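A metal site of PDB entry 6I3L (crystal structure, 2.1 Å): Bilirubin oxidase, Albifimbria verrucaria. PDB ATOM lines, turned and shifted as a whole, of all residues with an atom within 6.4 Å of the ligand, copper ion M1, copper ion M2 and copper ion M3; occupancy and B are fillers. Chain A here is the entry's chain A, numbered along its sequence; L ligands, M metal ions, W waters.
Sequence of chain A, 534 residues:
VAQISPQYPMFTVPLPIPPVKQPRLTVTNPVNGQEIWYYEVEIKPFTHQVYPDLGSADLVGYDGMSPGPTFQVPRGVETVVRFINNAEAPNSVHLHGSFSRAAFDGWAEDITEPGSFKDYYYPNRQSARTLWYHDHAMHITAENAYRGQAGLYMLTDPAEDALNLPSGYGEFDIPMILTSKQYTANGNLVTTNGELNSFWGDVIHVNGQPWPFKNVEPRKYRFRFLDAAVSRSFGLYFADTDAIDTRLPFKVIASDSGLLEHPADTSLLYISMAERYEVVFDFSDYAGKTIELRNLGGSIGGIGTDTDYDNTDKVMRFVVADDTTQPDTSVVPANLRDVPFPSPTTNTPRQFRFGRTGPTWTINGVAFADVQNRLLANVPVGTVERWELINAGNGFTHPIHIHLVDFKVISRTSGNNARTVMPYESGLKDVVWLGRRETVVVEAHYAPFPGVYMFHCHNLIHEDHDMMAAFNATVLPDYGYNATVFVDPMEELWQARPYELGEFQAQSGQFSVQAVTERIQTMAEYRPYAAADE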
ATOM      1  N   HIS A  94       0.276 -21.748  20.093  1.00  0.00           N
ATOM      2  CA  HIS A  94       1.674 -21.330  19.862  1.00  0.00           C
ATOM      3  C   HIS A  94       1.834 -19.849  20.197  1.00  0.00           C
ATOM      4  O   HIS A  94       1.090 -19.032  19.592  1.00  0.00           O
ATOM      5  CB  HIS A  94       2.051 -21.589  18.401  1.00  0.00           C
ATOM      6  CG  HIS A  94       3.366 -21.015  18.047  1.00  0.00           C
ATOM      7  ND1 HIS A  94       4.499 -21.332  18.759  1.00  0.00           N
ATOM      8  CD2 HIS A  94       3.735 -20.196  17.032  1.00  0.00           C
ATOM      9  CE1 HIS A  94       5.532 -20.732  18.196  1.00  0.00           C
ATOM     10  NE2 HIS A  94       5.071 -20.020  17.141  1.00  0.00           N
ATOM     11  N   LEU A  95       2.792 -19.524  21.075  1.00  0.00           N
ATOM     12  CA  LEU A  95       3.313 -18.156  21.304  1.00  0.00           C
ATOM     13  C   LEU A  95       4.429 -17.884  20.286  1.00  0.00           C
ATOM     14  O   LEU A  95       5.593 -18.322  20.488  1.00  0.00           O
ATOM     15  CB  LEU A  95       3.827 -17.993  22.743  1.00  0.00           C
ATOM     16  CG  LEU A  95       4.260 -16.585  23.139  1.00  0.00           C
ATOM     17  CD1 LEU A  95       3.163 -15.584  22.810  1.00  0.00           C
ATOM     18  CD2 LEU A  95       4.606 -16.505  24.622  1.00  0.00           C
ATOM     19  N   HIS A  96       4.066 -17.224  19.212  1.00  0.00           N
ATOM     20  CA  HIS A  96       4.973 -16.933  18.068  1.00  0.00           C
ATOM     21  C   HIS A  96       5.932 -15.803  18.485  1.00  0.00           C
ATOM     22  O   HIS A  96       5.465 -14.689  18.800  1.00  0.00           O
ATOM     23  CB  HIS A  96       4.092 -16.628  16.853  1.00  0.00           C
ATOM     24  CG  HIS A  96       4.847 -16.510  15.577  1.00  0.00           C
ATOM     25  ND1 HIS A  96       4.397 -17.062  14.413  1.00  0.00           N
ATOM     26  CD2 HIS A  96       6.032 -15.917  15.290  1.00  0.00           C
ATOM     27  CE1 HIS A  96       5.246 -16.793  13.447  1.00  0.00           C
ATOM     28  NE2 HIS A  96       6.257 -16.105  13.956  1.00  0.00           N
ATOM     29  N   GLY A  97       7.224 -16.089  18.525  1.00  0.00           N
ATOM     30  CA  GLY A  97       8.279 -15.131  18.908  1.00  0.00           C
ATOM     31  C   GLY A  97       8.955 -15.535  20.209  1.00  0.00           C
ATOM     32  O   GLY A  97       9.872 -14.807  20.603  1.00  0.00           O
ATOM     33  N   ASP A 105       5.199 -25.081  23.094  1.00  0.00           N
ATOM     34  CA  ASP A 105       5.422 -24.272  21.862  1.00  0.00           C
ATOM     35  C   ASP A 105       4.265 -24.408  20.859  1.00  0.00           C
ATOM     36  O   ASP A 105       4.328 -23.695  19.850  1.00  0.00           O
ATOM     37  CB  ASP A 105       6.696 -24.682  21.125  1.00  0.00           C
ATOM     38  CG  ASP A 105       7.182 -23.662  20.107  1.00  0.00           C
ATOM     39  OD1 ASP A 105       7.202 -22.444  20.450  1.00  0.00           O
ATOM     40  OD2 ASP A 105       7.536 -24.089  18.965  1.00  0.00           O
ATOM     41  N   GLY A 106       3.256 -25.246  21.104  1.00  0.00           N
ATOM     42  CA  GLY A 106       2.124 -25.461  20.182  1.00  0.00           C
ATOM     43  C   GLY A 106       2.470 -26.398  19.022  1.00  0.00           C
ATOM     44  O   GLY A 106       1.909 -26.213  17.908  1.00  0.00           O
ATOM     45  N   TRP A 132       2.761 -12.883  19.203  1.00  0.00           N
ATOM     46  CA  TRP A 132       1.328 -13.147  19.089  1.00  0.00           C
ATOM     47  C   TRP A 132       1.118 -14.624  19.389  1.00  0.00           C
ATOM     48  O   TRP A 132       2.050 -15.408  19.186  1.00  0.00           O
ATOM     49  CB  TRP A 132       0.791 -12.625  17.744  1.00  0.00           C
ATOM     50  CG  TRP A 132       1.277 -13.323  16.501  1.00  0.00           C
ATOM     51  CD1 TRP A 132       2.561 -13.462  16.058  1.00  0.00           C
ATOM     52  CD2 TRP A 132       0.440 -13.921  15.509  1.00  0.00           C
ATOM     53  NE1 TRP A 132       2.573 -14.148  14.879  1.00  0.00           N
ATOM     54  CE2 TRP A 132       1.283 -14.445  14.510  1.00  0.00           C
ATOM     55  CE3 TRP A 132      -0.939 -14.067  15.373  1.00  0.00           C
ATOM     56  CZ2 TRP A 132       0.788 -15.088  13.381  1.00  0.00           C
ATOM     57  CZ3 TRP A 132      -1.437 -14.722  14.272  1.00  0.00           C
ATOM     58  CH2 TRP A 132      -0.576 -15.227  13.293  1.00  0.00           C
ATOM     59  N   HIS A 134      -1.539 -17.945  18.940  1.00  0.00           N
ATOM     60  CA  HIS A 134      -2.553 -18.358  17.944  1.00  0.00           C
ATOM     61  C   HIS A 134      -2.624 -19.869  17.836  1.00  0.00           C
ATOM     62  O   HIS A 134      -1.702 -20.574  18.324  1.00  0.00           O
ATOM     63  CB  HIS A 134      -2.290 -17.722  16.572  1.00  0.00           C
ATOM     64  CG  HIS A 134      -1.035 -18.158  15.910  1.00  0.00           C
ATOM     65  ND1 HIS A 134      -0.906 -19.392  15.319  1.00  0.00           N
ATOM     66  CD2 HIS A 134       0.116 -17.514  15.693  1.00  0.00           C
ATOM     67  CE1 HIS A 134       0.285 -19.487  14.751  1.00  0.00           C
ATOM     68  NE2 HIS A 134       0.930 -18.361  14.975  1.00  0.00           N
ATOM     69  N   ASP A 135      -3.671 -20.332  17.163  1.00  0.00           N
ATOM     70  CA  ASP A 135      -3.910 -21.779  17.080  1.00  0.00           C
ATOM     71  C   ASP A 135      -2.913 -22.377  16.115  1.00  0.00           C
ATOM     72  O   ASP A 135      -2.504 -21.686  15.173  1.00  0.00           O
ATOM     73  CB  ASP A 135      -5.347 -22.125  16.685  1.00  0.00           C
ATOM     74  CG  ASP A 135      -5.531 -23.614  16.885  1.00  0.00           C
ATOM     75  OD1 ASP A 135      -5.377 -24.036  18.070  1.00  0.00           O
ATOM     76  OD2 ASP A 135      -5.661 -24.316  15.865  1.00  0.00           O
ATOM     77  N   HIS A 136      -2.502 -23.616  16.392  1.00  0.00           N
ATOM     78  CA  HIS A 136      -1.501 -24.356  15.588  1.00  0.00           C
ATOM     79  C   HIS A 136      -1.940 -25.822  15.430  1.00  0.00           C
ATOM     80  O   HIS A 136      -1.112 -26.620  15.035  1.00  0.00           O
ATOM     81  CB  HIS A 136      -0.126 -24.189  16.230  1.00  0.00           C
ATOM     82  CG  HIS A 136       1.001 -24.148  15.252  1.00  0.00           C
ATOM     83  ND1 HIS A 136       1.141 -25.101  14.255  1.00  0.00           N
ATOM     84  CD2 HIS A 136       2.032 -23.286  15.118  1.00  0.00           C
ATOM     85  CE1 HIS A 136       2.211 -24.824  13.526  1.00  0.00           C
ATOM     86  NE2 HIS A 136       2.785 -23.703  14.031  1.00  0.00           N
ATOM     87  N   ALA A 274       2.305 -13.469   9.504  1.00  0.00           N
ATOM     88  CA  ALA A 274       2.992 -13.755  10.789  1.00  0.00           C
ATOM     89  C   ALA A 274       4.122 -12.758  11.023  1.00  0.00           C
ATOM     90  O   ALA A 274       4.658 -12.750  12.112  1.00  0.00           O
ATOM     91  CB  ALA A 274       3.467 -15.185  10.868  1.00  0.00           C
ATOM     92  N   HIS A 401       8.596 -19.524   8.366  1.00  0.00           N
ATOM     93  CA  HIS A 401       8.759 -19.303   9.816  1.00  0.00           C
ATOM     94  C   HIS A 401       9.531 -20.472  10.384  1.00  0.00           C
ATOM     95  O   HIS A 401       9.199 -21.610  10.022  1.00  0.00           O
ATOM     96  CB  HIS A 401       7.393 -19.224  10.464  1.00  0.00           C
ATOM     97  CG  HIS A 401       7.466 -19.130  11.940  1.00  0.00           C
ATOM     98  ND1 HIS A 401       8.384 -18.326  12.580  1.00  0.00           N
ATOM     99  CD2 HIS A 401       6.705 -19.738  12.891  1.00  0.00           C
ATOM    100  CE1 HIS A 401       8.189 -18.400  13.880  1.00  0.00           C
ATOM    101  NE2 HIS A 401       7.157 -19.270  14.087  1.00  0.00           N
ATOM    102  N   ILE A 402      10.510 -20.177  11.231  1.00  0.00           N
ATOM    103  CA  ILE A 402      11.278 -21.196  11.987  1.00  0.00           C
ATOM    104  C   ILE A 402      11.029 -20.964  13.477  1.00  0.00           C
ATOM    105  O   ILE A 402      11.360 -19.867  13.985  1.00  0.00           O
ATOM    106  CB  ILE A 402      12.770 -21.152  11.631  1.00  0.00           C
ATOM    107  CG1 ILE A 402      13.001 -21.169  10.116  1.00  0.00           C
ATOM    108  CG2 ILE A 402      13.484 -22.313  12.335  1.00  0.00           C
ATOM    109  CD1 ILE A 402      14.447 -20.956   9.681  1.00  0.00           C
ATOM    110  N   HIS A 403      10.486 -21.978  14.165  1.00  0.00           N
ATOM    111  CA  HIS A 403      10.286 -21.932  15.642  1.00  0.00           C
ATOM    112  C   HIS A 403      11.641 -21.880  16.354  1.00  0.00           C
ATOM    113  O   HIS A 403      12.671 -22.089  15.709  1.00  0.00           O
ATOM    114  CB  HIS A 403       9.454 -23.111  16.141  1.00  0.00           C
ATOM    115  CG  HIS A 403       8.030 -23.018  15.737  1.00  0.00           C
ATOM    116  ND1 HIS A 403       7.009 -23.143  16.630  1.00  0.00           N
ATOM    117  CD2 HIS A 403       7.451 -22.849  14.518  1.00  0.00           C
ATOM    118  CE1 HIS A 403       5.864 -23.036  16.007  1.00  0.00           C
ATOM    119  NE2 HIS A 403       6.097 -22.857  14.700  1.00  0.00           N
ATOM    120  N   LEU A 404      11.597 -21.604  17.648  1.00  0.00           N
ATOM    121  CA  LEU A 404      12.718 -21.506  18.609  1.00  0.00           C
ATOM    122  C   LEU A 404      13.556 -20.238  18.351  1.00  0.00           C
ATOM    123  O   LEU A 404      13.759 -19.481  19.315  1.00  0.00           O
ATOM    124  CB  LEU A 404      13.586 -22.759  18.528  1.00  0.00           C
ATOM    125  CG  LEU A 404      14.897 -22.657  19.319  1.00  0.00           C
ATOM    126  CD1 LEU A 404      14.585 -22.540  20.810  1.00  0.00           C
ATOM    127  CD2 LEU A 404      15.820 -23.839  19.056  1.00  0.00           C
ATOM    128  N   ASP A 430      11.794 -13.836  12.569  1.00  0.00           N
ATOM    129  CA  ASP A 430      11.475 -15.282  12.682  1.00  0.00           C
ATOM    130  C   ASP A 430      10.550 -15.734  11.541  1.00  0.00           C
ATOM    131  O   ASP A 430      10.252 -16.938  11.482  1.00  0.00           O
ATOM    132  CB  ASP A 430      10.910 -15.610  14.061  1.00  0.00           C
ATOM    133  CG  ASP A 430       9.648 -14.863  14.445  1.00  0.00           C
ATOM    134  OD1 ASP A 430       8.824 -14.565  13.538  1.00  0.00           O
ATOM    135  OD2 ASP A 430       9.509 -14.610  15.665  1.00  0.00           O
ATOM    136  N   VAL A 431      10.114 -14.820  10.688  1.00  0.00           N
ATOM    137  CA  VAL A 431       9.389 -15.073   9.424  1.00  0.00           C
ATOM    138  C   VAL A 431      10.120 -14.308   8.326  1.00  0.00           C
ATOM    139  O   VAL A 431      10.511 -13.149   8.563  1.00  0.00           O
ATOM    140  CB  VAL A 431       7.920 -14.608   9.497  1.00  0.00           C
ATOM    141  CG1 VAL A 431       7.132 -14.943   8.236  1.00  0.00           C
ATOM    142  CG2 VAL A 431       7.220 -15.151  10.720  1.00  0.00           C
ATOM    143  N   MET A 454       8.971 -27.006  14.974  1.00  0.00           N
ATOM    144  CA  MET A 454       8.421 -26.925  13.615  1.00  0.00           C
ATOM    145  C   MET A 454       9.092 -25.792  12.838  1.00  0.00           C
ATOM    146  O   MET A 454       9.669 -24.895  13.428  1.00  0.00           O
ATOM    147  CB  MET A 454       6.909 -26.718  13.656  1.00  0.00           C
ATOM    148  CG  MET A 454       6.165 -27.897  14.287  1.00  0.00           C
ATOM    149  SD  MET A 454       4.385 -27.559  14.497  1.00  0.00           S
ATOM    150  CE  MET A 454       4.399 -26.105  15.539  1.00  0.00           C
ATOM    151  N   PHE A 455       9.074 -25.915  11.510  1.00  0.00           N
ATOM    152  CA  PHE A 455       9.315 -24.813  10.568  1.00  0.00           C
ATOM    153  C   PHE A 455       8.402 -25.055   9.360  1.00  0.00           C
ATOM    154  O   PHE A 455       8.000 -26.186   9.122  1.00  0.00           O
ATOM    155  CB  PHE A 455      10.794 -24.659  10.211  1.00  0.00           C
ATOM    156  CG  PHE A 455      11.383 -25.700   9.289  1.00  0.00           C
ATOM    157  CD1 PHE A 455      11.739 -26.952   9.771  1.00  0.00           C
ATOM    158  CD2 PHE A 455      11.601 -25.417   7.967  1.00  0.00           C
ATOM    159  CE1 PHE A 455      12.325 -27.890   8.933  1.00  0.00           C
ATOM    160  CE2 PHE A 455      12.203 -26.341   7.137  1.00  0.00           C
ATOM    161  CZ  PHE A 455      12.567 -27.572   7.617  1.00  0.00           C
ATOM    162  N   HIS A 456       7.972 -23.994   8.718  1.00  0.00           N
ATOM    163  CA  HIS A 456       6.851 -24.092   7.757  1.00  0.00           C
ATOM    164  C   HIS A 456       6.619 -22.753   7.076  1.00  0.00           C
ATOM    165  O   HIS A 456       7.092 -21.673   7.552  1.00  0.00           O
ATOM    166  CB  HIS A 456       5.573 -24.557   8.461  1.00  0.00           C
ATOM    167  CG  HIS A 456       5.154 -23.701   9.602  1.00  0.00           C
ATOM    168  ND1 HIS A 456       4.228 -22.681   9.475  1.00  0.00           N
ATOM    169  CD2 HIS A 456       5.539 -23.706  10.904  1.00  0.00           C
ATOM    170  CE1 HIS A 456       4.049 -22.101  10.645  1.00  0.00           C
ATOM    171  NE2 HIS A 456       4.850 -22.721  11.542  1.00  0.00           N
ATOM    172  N   HIS A 458       3.839 -19.923   6.564  1.00  0.00           N
ATOM    173  CA  HIS A 458       2.759 -19.338   7.394  1.00  0.00           C
ATOM    174  C   HIS A 458       1.588 -18.830   6.569  1.00  0.00           C
ATOM    175  O   HIS A 458       0.667 -18.180   7.196  1.00  0.00           O
ATOM    176  CB  HIS A 458       3.307 -18.220   8.295  1.00  0.00           C
ATOM    177  CG  HIS A 458       2.717 -18.214   9.673  1.00  0.00           C
ATOM    178  ND1 HIS A 458       1.416 -17.823   9.901  1.00  0.00           N
ATOM    179  CD2 HIS A 458       3.264 -18.473  10.886  1.00  0.00           C
ATOM    180  CE1 HIS A 458       1.172 -17.888  11.197  1.00  0.00           C
ATOM    181  NE2 HIS A 458       2.294 -18.259  11.832  1.00  0.00           N
ATOM    182  N   LEU A 460      -1.559 -20.095   5.896  1.00  0.00           N
ATOM    183  CA  LEU A 460      -2.124 -21.175   6.751  1.00  0.00           C
ATOM    184  C   LEU A 460      -2.753 -22.252   5.855  1.00  0.00           C
ATOM    185  O   LEU A 460      -2.824 -23.417   6.296  1.00  0.00           O
ATOM    186  CB  LEU A 460      -3.094 -20.592   7.778  1.00  0.00           C
ATOM    187  CG  LEU A 460      -2.477 -19.580   8.755  1.00  0.00           C
ATOM    188  CD1 LEU A 460      -3.534 -19.028   9.693  1.00  0.00           C
ATOM    189  CD2 LEU A 460      -1.326 -20.173   9.554  1.00  0.00           C
ATOM    190  N   GLU A 463       0.331 -24.361   4.948  1.00  0.00           N
ATOM    191  CA  GLU A 463       0.744 -25.040   6.205  1.00  0.00           C
ATOM    192  C   GLU A 463      -0.162 -26.262   6.473  1.00  0.00           C
ATOM    193  O   GLU A 463       0.372 -27.316   6.828  1.00  0.00           O
ATOM    194  CB  GLU A 463       0.657 -24.037   7.359  1.00  0.00           C
ATOM    195  CG  GLU A 463       1.180 -24.565   8.679  1.00  0.00           C
ATOM    196  CD  GLU A 463       0.951 -23.601   9.832  1.00  0.00           C
ATOM    197  OE1 GLU A 463       1.044 -22.358   9.588  1.00  0.00           O
ATOM    198  OE2 GLU A 463       0.684 -24.091  10.958  1.00  0.00           O
ATOM    199  N   MET A 468       5.094 -28.088   6.052  1.00  0.00           N
ATOM    200  CA  MET A 468       5.591 -28.000   7.438  1.00  0.00           C
ATOM    201  C   MET A 468       6.430 -29.231   7.697  1.00  0.00           C
ATOM    202  O   MET A 468       6.141 -30.271   7.130  1.00  0.00           O
ATOM    203  CB  MET A 468       4.410 -27.926   8.411  1.00  0.00           C
ATOM    204  CG  MET A 468       4.802 -27.750   9.873  1.00  0.00           C
ATOM    205  SD  MET A 468       3.423 -26.966  10.743  1.00  0.00           S
ATOM    206  CE  MET A 468       2.250 -28.323  10.784  1.00  0.00           C
HETATM  207  O1  LIG L   1       3.026 -20.403  13.536  1.00  0.00           O
HETATM  208  O2  LIG L   1       4.206 -20.418  14.156  1.00  0.00           O
HETATM  209 CU    CU M   1       2.715 -18.040  14.008  1.00  0.00          CU
HETATM  210 CU    CU M   2       4.412 -22.598  13.570  1.00  0.00          CU
HETATM  211 CU    CU M   3       6.100 -19.640  15.614  1.00  0.00          CU
HETATM  212  O   HOH W   1       1.042 -21.370  12.111  1.00  0.00           O
HETATM  213  O   HOH W   2       8.383 -18.727  17.532  1.00  0.00           O
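Copper ion M3 is bound by NE2 of His 94 (1.9 Å), NE2 of His 401 (1.9 Å) and O2 of the ligand (2.5 Å).
Copper ion M3 has three donor atoms within binding distance.
N of His 403 sits at hydrogen-bond distance from O of Met 454 (3.1 Å).
The backbone NH of His 401 is in hydrogen-bond range of the backbone carbonyl oxygen of His 456 (2.7 Å).
A ring nitrogen (NE2) of His 96 lies close to a ring nitrogen (ND1) of His 401 (3.4 Å).
The backbone NH (N) of His 94 is in hydrogen-bond range of the backbone carbonyl oxygen (O) of His 134, 2.9 Å away.
OE1 of Glu 463 sits close to ND1 of His 456, at 3.2 Å.
A ring nitrogen (ND1) of His 401 sits at hydrogen-bond distance from the backbone carbonyl oxygen (O) of Asp 430 (2.6 Å).
The backbone carbonyl oxygen (O) of Asp 105 lies within hydrogen-bond range of a ring nitrogen (ND1) of His 94 (2.6 Å).
A ring nitrogen (ND1) of His 136 sits close to the side-chain carboxylate (OE2) of Glu 463 (3.5 Å).
Copper ion M1 is bound by a ring nitrogen (ND1) of His 96 (2.0 Å).
NE2 of His 134 is bound to copper ion M1 (2.1 Å).
A ring nitrogen (NE2) of His 458 binds copper ion M1 (2.2 Å).
An oxygen (O1) of the ligand is bound to copper ion M1, 2.4 Å away.
Copper ion M1 has four donor atoms within binding distance.
Four residues have an atom within 4 Å of copper ion M2: His 136, His 401, His 403 and His 456.
The nearest printed residue that does not touch copper ion M2 is Met 454 (4.02 Å).
Copper ion M2 is bound by NE2 of His 136 (2.0 Å), NE2 of His 403 (2.0 Å), NE2 of His 456 (2.1 Å) and O2 of the ligand (2.3 Å).
Trp 132 touches copper ion M1 (CZ2 to CU, 3.6 Å).
Within 4 Å of copper ion M1: His 94, His 96, Trp 132, His 134 and His 458.
The nearest printed residue that does not touch copper ion M1 is Ala 274 (4.3 Å).
Of the 24 residues printed, 8 come within 4 Å of the ligand.
Along chain A the residues within 4 Å of the ligand span positions 94 to 458.
The nearest printed residue that does not touch the ligand is Glu 463 (4.8 Å).
Four residues have an atom within 4 Å of copper ion M3: His 94, His 96, His 401 and His 403.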
